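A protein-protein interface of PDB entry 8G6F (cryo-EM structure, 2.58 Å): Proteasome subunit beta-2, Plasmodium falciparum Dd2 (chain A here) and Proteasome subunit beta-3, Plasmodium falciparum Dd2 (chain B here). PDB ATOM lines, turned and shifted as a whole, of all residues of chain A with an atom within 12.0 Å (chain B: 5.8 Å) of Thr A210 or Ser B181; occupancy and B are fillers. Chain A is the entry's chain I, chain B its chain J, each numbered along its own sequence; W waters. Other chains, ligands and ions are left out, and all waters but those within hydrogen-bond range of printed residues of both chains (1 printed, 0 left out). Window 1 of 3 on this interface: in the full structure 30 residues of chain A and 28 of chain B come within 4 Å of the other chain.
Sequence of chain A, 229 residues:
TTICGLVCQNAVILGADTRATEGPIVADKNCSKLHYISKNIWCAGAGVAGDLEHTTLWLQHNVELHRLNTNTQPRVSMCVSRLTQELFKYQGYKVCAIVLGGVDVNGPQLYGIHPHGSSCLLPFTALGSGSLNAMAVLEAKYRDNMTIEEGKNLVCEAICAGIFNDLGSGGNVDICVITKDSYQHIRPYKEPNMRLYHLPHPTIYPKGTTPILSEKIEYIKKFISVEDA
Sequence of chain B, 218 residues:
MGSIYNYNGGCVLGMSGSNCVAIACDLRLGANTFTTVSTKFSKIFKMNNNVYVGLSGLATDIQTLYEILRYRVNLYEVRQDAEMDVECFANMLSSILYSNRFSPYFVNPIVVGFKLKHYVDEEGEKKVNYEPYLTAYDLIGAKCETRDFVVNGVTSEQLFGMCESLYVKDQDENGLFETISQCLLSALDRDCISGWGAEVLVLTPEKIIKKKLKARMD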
ATOM      1  N   THR A 203      18.011 -22.380  -6.950  1.00  0.00           N
ATOM      2  CA  THR A 203      16.796 -23.185  -7.040  1.00  0.00           C
ATOM      3  C   THR A 203      15.637 -22.268  -7.401  1.00  0.00           C
ATOM      4  O   THR A 203      15.141 -21.513  -6.564  1.00  0.00           O
ATOM      5  CB  THR A 203      16.540 -23.922  -5.732  1.00  0.00           C
ATOM      6  OG1 THR A 203      17.531 -24.942  -5.557  1.00  0.00           O
ATOM      7  CG2 THR A 203      15.158 -24.557  -5.735  1.00  0.00           C
ATOM      8  N   ILE A 204      15.207 -22.336  -8.656  1.00  0.00           N
ATOM      9  CA  ILE A 204      14.046 -21.599  -9.137  1.00  0.00           C
ATOM     10  C   ILE A 204      12.878 -22.571  -9.194  1.00  0.00           C
ATOM     11  O   ILE A 204      12.942 -23.591  -9.890  1.00  0.00           O
ATOM     12  CB  ILE A 204      14.307 -20.969 -10.514  1.00  0.00           C
ATOM     13  CG1 ILE A 204      15.678 -20.288 -10.558  1.00  0.00           C
ATOM     14  CG2 ILE A 204      13.212 -19.976 -10.856  1.00  0.00           C
ATOM     15  CD1 ILE A 204      15.800 -19.084  -9.656  1.00  0.00           C
ATOM     16  N   TYR A 205      11.821 -22.266  -8.460  1.00  0.00           N
ATOM     17  CA  TYR A 205      10.660 -23.138  -8.447  1.00  0.00           C
ATOM     18  C   TYR A 205       9.888 -23.009  -9.757  1.00  0.00           C
ATOM     19  O   TYR A 205       9.672 -21.894 -10.242  1.00  0.00           O
ATOM     20  CB  TYR A 205       9.754 -22.794  -7.271  1.00  0.00           C
ATOM     21  CG  TYR A 205      10.332 -23.193  -5.941  1.00  0.00           C
ATOM     22  CD1 TYR A 205      10.349 -24.520  -5.543  1.00  0.00           C
ATOM     23  CD2 TYR A 205      10.868 -22.248  -5.086  1.00  0.00           C
ATOM     24  CE1 TYR A 205      10.877 -24.892  -4.336  1.00  0.00           C
ATOM     25  CE2 TYR A 205      11.398 -22.613  -3.872  1.00  0.00           C
ATOM     26  CZ  TYR A 205      11.399 -23.937  -3.504  1.00  0.00           C
ATOM     27  OH  TYR A 205      11.925 -24.310  -2.296  1.00  0.00           O
ATOM     28  N   PRO A 206       9.461 -24.120 -10.356  1.00  0.00           N
ATOM     29  CA  PRO A 206       8.624 -24.020 -11.553  1.00  0.00           C
ATOM     30  C   PRO A 206       7.305 -23.334 -11.237  1.00  0.00           C
ATOM     31  O   PRO A 206       6.767 -23.450 -10.137  1.00  0.00           O
ATOM     32  CB  PRO A 206       8.416 -25.479 -11.972  1.00  0.00           C
ATOM     33  CG  PRO A 206       8.674 -26.273 -10.756  1.00  0.00           C
ATOM     34  CD  PRO A 206       9.689 -25.520  -9.963  1.00  0.00           C
ATOM     35  N   LYS A 207       6.792 -22.601 -12.219  1.00  0.00           N
ATOM     36  CA  LYS A 207       5.546 -21.879 -12.022  1.00  0.00           C
ATOM     37  C   LYS A 207       4.404 -22.851 -11.756  1.00  0.00           C
ATOM     38  O   LYS A 207       4.320 -23.921 -12.366  1.00  0.00           O
ATOM     39  CB  LYS A 207       5.231 -21.022 -13.245  1.00  0.00           C
ATOM     40  CG  LYS A 207       4.179 -19.964 -12.986  1.00  0.00           C
ATOM     41  CD  LYS A 207       3.559 -19.461 -14.273  1.00  0.00           C
ATOM     42  CE  LYS A 207       2.870 -18.122 -14.060  1.00  0.00           C
ATOM     43  NZ  LYS A 207       1.853 -18.176 -12.969  1.00  0.00           N
ATOM     44  N   GLY A 208       3.520 -22.470 -10.839  1.00  0.00           N
ATOM     45  CA  GLY A 208       2.380 -23.294 -10.508  1.00  0.00           C
ATOM     46  C   GLY A 208       2.668 -24.433  -9.563  1.00  0.00           C
ATOM     47  O   GLY A 208       1.787 -25.271  -9.348  1.00  0.00           O
ATOM     48  N   THR A 209       3.872 -24.497  -8.990  1.00  0.00           N
ATOM     49  CA  THR A 209       4.209 -25.601  -8.100  1.00  0.00           C
ATOM     50  C   THR A 209       3.528 -25.458  -6.746  1.00  0.00           C
ATOM     51  O   THR A 209       3.290 -26.461  -6.067  1.00  0.00           O
ATOM     52  CB  THR A 209       5.725 -25.691  -7.925  1.00  0.00           C
ATOM     53  OG1 THR A 209       6.081 -27.000  -7.472  1.00  0.00           O
ATOM     54  CG2 THR A 209       6.219 -24.668  -6.918  1.00  0.00           C
ATOM     55  N   THR A 210       3.216 -24.235  -6.333  1.00  0.00           N
ATOM     56  CA  THR A 210       2.540 -24.008  -5.064  1.00  0.00           C
ATOM     57  C   THR A 210       1.034 -24.102  -5.266  1.00  0.00           C
ATOM     58  O   THR A 210       0.489 -23.374  -6.105  1.00  0.00           O
ATOM     59  CB  THR A 210       2.898 -22.644  -4.500  1.00  0.00           C
ATOM     60  OG1 THR A 210       4.318 -22.463  -4.534  1.00  0.00           O
ATOM     61  CG2 THR A 210       2.415 -22.515  -3.069  1.00  0.00           C
ATOM     62  N   PRO A 211       0.327 -24.969  -4.542  1.00  0.00           N
ATOM     63  CA  PRO A 211      -1.134 -24.990  -4.650  1.00  0.00           C
ATOM     64  C   PRO A 211      -1.764 -23.841  -3.881  1.00  0.00           C
ATOM     65  O   PRO A 211      -1.338 -23.497  -2.777  1.00  0.00           O
ATOM     66  CB  PRO A 211      -1.509 -26.344  -4.042  1.00  0.00           C
ATOM     67  CG  PRO A 211      -0.440 -26.615  -3.070  1.00  0.00           C
ATOM     68  CD  PRO A 211       0.818 -26.003  -3.616  1.00  0.00           C
ATOM     69  N   ILE A 212      -2.793 -23.246  -4.475  1.00  0.00           N
ATOM     70  CA  ILE A 212      -3.470 -22.101  -3.884  1.00  0.00           C
ATOM     71  C   ILE A 212      -4.952 -22.413  -3.764  1.00  0.00           C
ATOM     72  O   ILE A 212      -5.508 -23.200  -4.533  1.00  0.00           O
ATOM     73  CB  ILE A 212      -3.248 -20.810  -4.701  1.00  0.00           C
ATOM     74  CG1 ILE A 212      -4.001 -20.878  -6.027  1.00  0.00           C
ATOM     75  CG2 ILE A 212      -1.767 -20.586  -4.944  1.00  0.00           C
ATOM     76  CD1 ILE A 212      -3.616 -19.791  -6.998  1.00  0.00           C
ATOM     77  N   LEU A 213      -5.589 -21.790  -2.777  1.00  0.00           N
ATOM     78  CA  LEU A 213      -7.024 -21.928  -2.580  1.00  0.00           C
ATOM     79  C   LEU A 213      -7.812 -20.878  -3.347  1.00  0.00           C
ATOM     80  O   LEU A 213      -8.834 -21.198  -3.959  1.00  0.00           O
ATOM     81  CB  LEU A 213      -7.364 -21.824  -1.092  1.00  0.00           C
ATOM     82  CG  LEU A 213      -6.956 -23.011  -0.230  1.00  0.00           C
ATOM     83  CD1 LEU A 213      -7.174 -22.680   1.224  1.00  0.00           C
ATOM     84  CD2 LEU A 213      -7.732 -24.251  -0.627  1.00  0.00           C
ATOM     85  N   SER A 214      -7.354 -19.631  -3.324  1.00  0.00           N
ATOM     86  CA  SER A 214      -8.071 -18.540  -3.962  1.00  0.00           C
ATOM     87  C   SER A 214      -7.070 -17.487  -4.408  1.00  0.00           C
ATOM     88  O   SER A 214      -5.945 -17.422  -3.911  1.00  0.00           O
ATOM     89  CB  SER A 214      -9.109 -17.929  -3.020  1.00  0.00           C
ATOM     90  OG  SER A 214      -8.483 -17.220  -1.972  1.00  0.00           O
ATOM     91  N   GLU A 215      -7.497 -16.665  -5.361  1.00  0.00           N
ATOM     92  CA  GLU A 215      -6.654 -15.605  -5.898  1.00  0.00           C
ATOM     93  C   GLU A 215      -7.531 -14.411  -6.221  1.00  0.00           C
ATOM     94  O   GLU A 215      -8.390 -14.494  -7.100  1.00  0.00           O
ATOM     95  CB  GLU A 215      -5.907 -16.075  -7.145  1.00  0.00           C
ATOM     96  CG  GLU A 215      -5.102 -14.991  -7.833  1.00  0.00           C
ATOM     97  CD  GLU A 215      -4.403 -15.493  -9.078  1.00  0.00           C
ATOM     98  OE1 GLU A 215      -4.338 -16.727  -9.265  1.00  0.00           O
ATOM     99  OE2 GLU A 215      -3.916 -14.658  -9.869  1.00  0.00           O
ATOM    100  N   LEU B 176       8.897 -14.621  -7.378  1.00  0.00           N
ATOM    101  CA  LEU B 176       8.883 -14.115  -6.013  1.00  0.00           C
ATOM    102  C   LEU B 176       7.767 -14.758  -5.204  1.00  0.00           C
ATOM    103  O   LEU B 176       7.975 -15.154  -4.051  1.00  0.00           O
ATOM    104  CB  LEU B 176       8.735 -12.595  -6.032  1.00  0.00           C
ATOM    105  CG  LEU B 176       8.522 -11.893  -4.694  1.00  0.00           C
ATOM    106  CD1 LEU B 176       9.711 -12.092  -3.791  1.00  0.00           C
ATOM    107  CD2 LEU B 176       8.271 -10.429  -4.924  1.00  0.00           C
ATOM    108  N   PHE B 177       6.576 -14.876  -5.790  1.00  0.00           N
ATOM    109  CA  PHE B 177       5.474 -15.528  -5.098  1.00  0.00           C
ATOM    110  C   PHE B 177       5.804 -16.982  -4.803  1.00  0.00           C
ATOM    111  O   PHE B 177       5.577 -17.470  -3.691  1.00  0.00           O
ATOM    112  CB  PHE B 177       4.196 -15.436  -5.928  1.00  0.00           C
ATOM    113  CG  PHE B 177       3.187 -16.482  -5.579  1.00  0.00           C
ATOM    114  CD1 PHE B 177       2.378 -16.335  -4.468  1.00  0.00           C
ATOM    115  CD2 PHE B 177       3.059 -17.623  -6.345  1.00  0.00           C
ATOM    116  CE1 PHE B 177       1.464 -17.299  -4.134  1.00  0.00           C
ATOM    117  CE2 PHE B 177       2.145 -18.591  -6.013  1.00  0.00           C
ATOM    118  CZ  PHE B 177       1.346 -18.430  -4.910  1.00  0.00           C
ATOM    119  N   GLU B 178       6.345 -17.697  -5.791  1.00  0.00           N
ATOM    120  CA  GLU B 178       6.665 -19.101  -5.559  1.00  0.00           C
ATOM    121  C   GLU B 178       7.688 -19.247  -4.444  1.00  0.00           C
ATOM    122  O   GLU B 178       7.528 -20.086  -3.550  1.00  0.00           O
ATOM    123  CB  GLU B 178       7.175 -19.746  -6.845  1.00  0.00           C
ATOM    124  CG  GLU B 178       6.125 -19.846  -7.932  1.00  0.00           C
ATOM    125  CD  GLU B 178       4.996 -20.783  -7.567  1.00  0.00           C
ATOM    126  OE1 GLU B 178       5.099 -21.459  -6.525  1.00  0.00           O
ATOM    127  OE2 GLU B 178       3.998 -20.834  -8.311  1.00  0.00           O
ATOM    128  N   THR B 179       8.732 -18.418  -4.460  1.00  0.00           N
ATOM    129  CA  THR B 179       9.777 -18.521  -3.450  1.00  0.00           C
ATOM    130  C   THR B 179       9.235 -18.207  -2.063  1.00  0.00           C
ATOM    131  O   THR B 179       9.483 -18.947  -1.106  1.00  0.00           O
ATOM    132  CB  THR B 179      10.927 -17.579  -3.794  1.00  0.00           C
ATOM    133  OG1 THR B 179      11.420 -17.886  -5.102  1.00  0.00           O
ATOM    134  CG2 THR B 179      12.052 -17.721  -2.787  1.00  0.00           C
ATOM    135  N   ILE B 180       8.503 -17.100  -1.928  1.00  0.00           N
ATOM    136  CA  ILE B 180       8.029 -16.704  -0.609  1.00  0.00           C
ATOM    137  C   ILE B 180       7.034 -17.721  -0.073  1.00  0.00           C
ATOM    138  O   ILE B 180       7.063 -18.069   1.113  1.00  0.00           O
ATOM    139  CB  ILE B 180       7.432 -15.286  -0.651  1.00  0.00           C
ATOM    140  CG1 ILE B 180       7.190 -14.782   0.773  1.00  0.00           C
ATOM    141  CG2 ILE B 180       6.148 -15.260  -1.460  1.00  0.00           C
ATOM    142  CD1 ILE B 180       6.942 -13.310   0.867  1.00  0.00           C
ATOM    143  N   SER B 181       6.135 -18.215  -0.927  1.00  0.00           N
ATOM    144  CA  SER B 181       5.169 -19.206  -0.475  1.00  0.00           C
ATOM    145  C   SER B 181       5.855 -20.501  -0.069  1.00  0.00           C
ATOM    146  O   SER B 181       5.479 -21.115   0.934  1.00  0.00           O
ATOM    147  CB  SER B 181       4.134 -19.456  -1.565  1.00  0.00           C
ATOM    148  OG  SER B 181       4.719 -19.343  -2.846  1.00  0.00           O
ATOM    149  N   GLN B 182       6.861 -20.940  -0.828  1.00  0.00           N
ATOM    150  CA  GLN B 182       7.574 -22.153  -0.451  1.00  0.00           C
ATOM    151  C   GLN B 182       8.293 -21.976   0.876  1.00  0.00           C
ATOM    152  O   GLN B 182       8.242 -22.858   1.743  1.00  0.00           O
ATOM    153  CB  GLN B 182       8.560 -22.541  -1.549  1.00  0.00           C
ATOM    154  CG  GLN B 182       7.921 -23.230  -2.742  1.00  0.00           C
ATOM    155  CD  GLN B 182       7.096 -24.427  -2.346  1.00  0.00           C
ATOM    156  OE1 GLN B 182       7.480 -25.190  -1.465  1.00  0.00           O
ATOM    157  NE2 GLN B 182       5.954 -24.597  -2.988  1.00  0.00           N
ATOM    158  N   CYS B 183       8.964 -20.838   1.056  1.00  0.00           N
ATOM    159  CA  CYS B 183       9.630 -20.568   2.323  1.00  0.00           C
ATOM    160  C   CYS B 183       8.637 -20.614   3.476  1.00  0.00           C
ATOM    161  O   CYS B 183       8.874 -21.281   4.490  1.00  0.00           O
ATOM    162  CB  CYS B 183      10.323 -19.206   2.265  1.00  0.00           C
ATOM    163  SG  CYS B 183      11.779 -19.141   1.204  1.00  0.00           S
ATOM    164  N   LEU B 184       7.509 -19.918   3.329  1.00  0.00           N
ATOM    165  CA  LEU B 184       6.535 -19.861   4.411  1.00  0.00           C
ATOM    166  C   LEU B 184       5.961 -21.237   4.713  1.00  0.00           C
ATOM    167  O   LEU B 184       5.817 -21.608   5.879  1.00  0.00           O
ATOM    168  CB  LEU B 184       5.415 -18.884   4.059  1.00  0.00           C
ATOM    169  CG  LEU B 184       4.404 -18.615   5.177  1.00  0.00           C
ATOM    170  CD1 LEU B 184       4.976 -17.659   6.206  1.00  0.00           C
ATOM    171  CD2 LEU B 184       3.113 -18.073   4.618  1.00  0.00           C
ATOM    172  N   LEU B 185       5.622 -22.008   3.681  1.00  0.00           N
ATOM    173  CA  LEU B 185       5.006 -23.308   3.916  1.00  0.00           C
ATOM    174  C   LEU B 185       5.981 -24.269   4.578  1.00  0.00           C
ATOM    175  O   LEU B 185       5.617 -24.979   5.522  1.00  0.00           O
ATOM    176  CB  LEU B 185       4.486 -23.884   2.601  1.00  0.00           C
ATOM    177  CG  LEU B 185       3.250 -23.188   2.030  1.00  0.00           C
ATOM    178  CD1 LEU B 185       2.974 -23.657   0.617  1.00  0.00           C
ATOM    179  CD2 LEU B 185       2.045 -23.427   2.913  1.00  0.00           C
ATOM    180  N   SER B 186       7.228 -24.298   4.111  1.00  0.00           N
ATOM    181  CA  SER B 186       8.210 -25.187   4.717  1.00  0.00           C
ATOM    182  C   SER B 186       8.509 -24.784   6.154  1.00  0.00           C
ATOM    183  O   SER B 186       8.685 -25.648   7.019  1.00  0.00           O
ATOM    184  CB  SER B 186       9.483 -25.195   3.882  1.00  0.00           C
ATOM    185  OG  SER B 186       9.206 -25.630   2.567  1.00  0.00           O
ATOM    186  N   VAL B 200      -0.666 -14.669   1.216  1.00  0.00           N
ATOM    187  CA  VAL B 200       0.477 -14.078   0.527  1.00  0.00           C
ATOM    188  C   VAL B 200      -0.020 -12.932  -0.341  1.00  0.00           C
ATOM    189  O   VAL B 200      -0.908 -13.122  -1.178  1.00  0.00           O
ATOM    190  CB  VAL B 200       1.231 -15.109  -0.327  1.00  0.00           C
ATOM    191  CG1 VAL B 200       2.466 -14.483  -0.951  1.00  0.00           C
ATOM    192  CG2 VAL B 200       1.609 -16.306   0.511  1.00  0.00           C
ATOM    193  N   LEU B 213      -3.044 -19.825   0.314  1.00  0.00           N
ATOM    194  CA  LEU B 213      -2.336 -21.044  -0.034  1.00  0.00           C
ATOM    195  C   LEU B 213      -3.052 -22.256   0.534  1.00  0.00           C
ATOM    196  O   LEU B 213      -3.597 -22.212   1.638  1.00  0.00           O
ATOM    197  CB  LEU B 213      -0.903 -21.003   0.495  1.00  0.00           C
ATOM    198  CG  LEU B 213      -0.051 -19.809   0.073  1.00  0.00           C
ATOM    199  CD1 LEU B 213       1.356 -19.981   0.597  1.00  0.00           C
ATOM    200  CD2 LEU B 213      -0.052 -19.642  -1.437  1.00  0.00           C
HETATM  201  O   HOH W   1      13.772 -20.246  -4.691  1.00  0.00           O
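OE2 of Glu B178 is in hydrogen-bond range of N of Gly A208, at 3.0 Å. The side-chain amide nitrogen (NE2) of Gln B182 lies within hydrogen-bond range of the side-chain hydroxyl (OG1) of Thr A210 (3.1 Å). The side-chain carboxylate (OE1) of Glu B178 sits close to the backbone NH (N) of Thr A210 (3.4 Å).
The side-chain hydroxyl (OG) of Ser B181 lies within hydrogen-bond range of the backbone carbonyl oxygen (O) of Glu B178 (3.0 Å). The backbone carbonyl oxygen (O) of Gln B182 is in hydrogen-bond range of the side-chain hydroxyl (OG) of Ser B186, 3.0 Å away.
Among the printed residues, pairs that only touch across the chains: Tyr A205 with Gln B182 (3.6 Å), Thr A209 with Glu B178 (3.4 Å), Thr A209 with Gln B182 (3.9 Å), Thr A210 with Ser B181 (3.6 Å), Thr A210 with Leu B185 (3.9 Å), Pro A211 with Leu B213 (3.8 Å), Ile A212 with Phe B177 (3.8 Å) and Leu A213 with Leu B213 (3.6 Å).
Thr A210 touches just these residues of chain B: Glu B178, Ser B181, Gln B182 and Leu B185. Printed residues of chain B within 4 Å of Pro A211: Leu B213. Of the printed residues of chain B, Ile A212 touches Phe B177 (3.8 Å). Of the printed residues of chain B, Leu A213 touches Leu B213 (3.6 Å). Glu A215 touches none of the printed residues of chain B. Phe B177 touches just one residue of chain A: Ile A212. Of the printed residues of chain A, Glu B178 touches Gly A208, Thr A209 and Thr A210. No residue of chain A comes within 4 Å of Thr B179. No residue of chain A comes within 4 Å of Ile B180. Ser B181 touches just one residue of chain A: Thr A210 (3.6 Å). Gln B182 touches three residues of chain A. No residue of chain A comes within 4 Å of Cys B183. Leu B185 touches just one residue of chain A: Thr A210. The nearest printed residue of chain A that does not touch Ser B181 is Thr A209 (6.9 Å).
Among the printed residues, no Asp or Glu carboxylate lies within 4 Å of a Lys or Arg side-chain nitrogen of the other chain.
Water W1 lies within hydrogen-bond range of the backbone carbonyl oxygen of Thr A203 (2.6 Å) and the side-chain hydroxyl of Thr B179 (3.4 Å).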
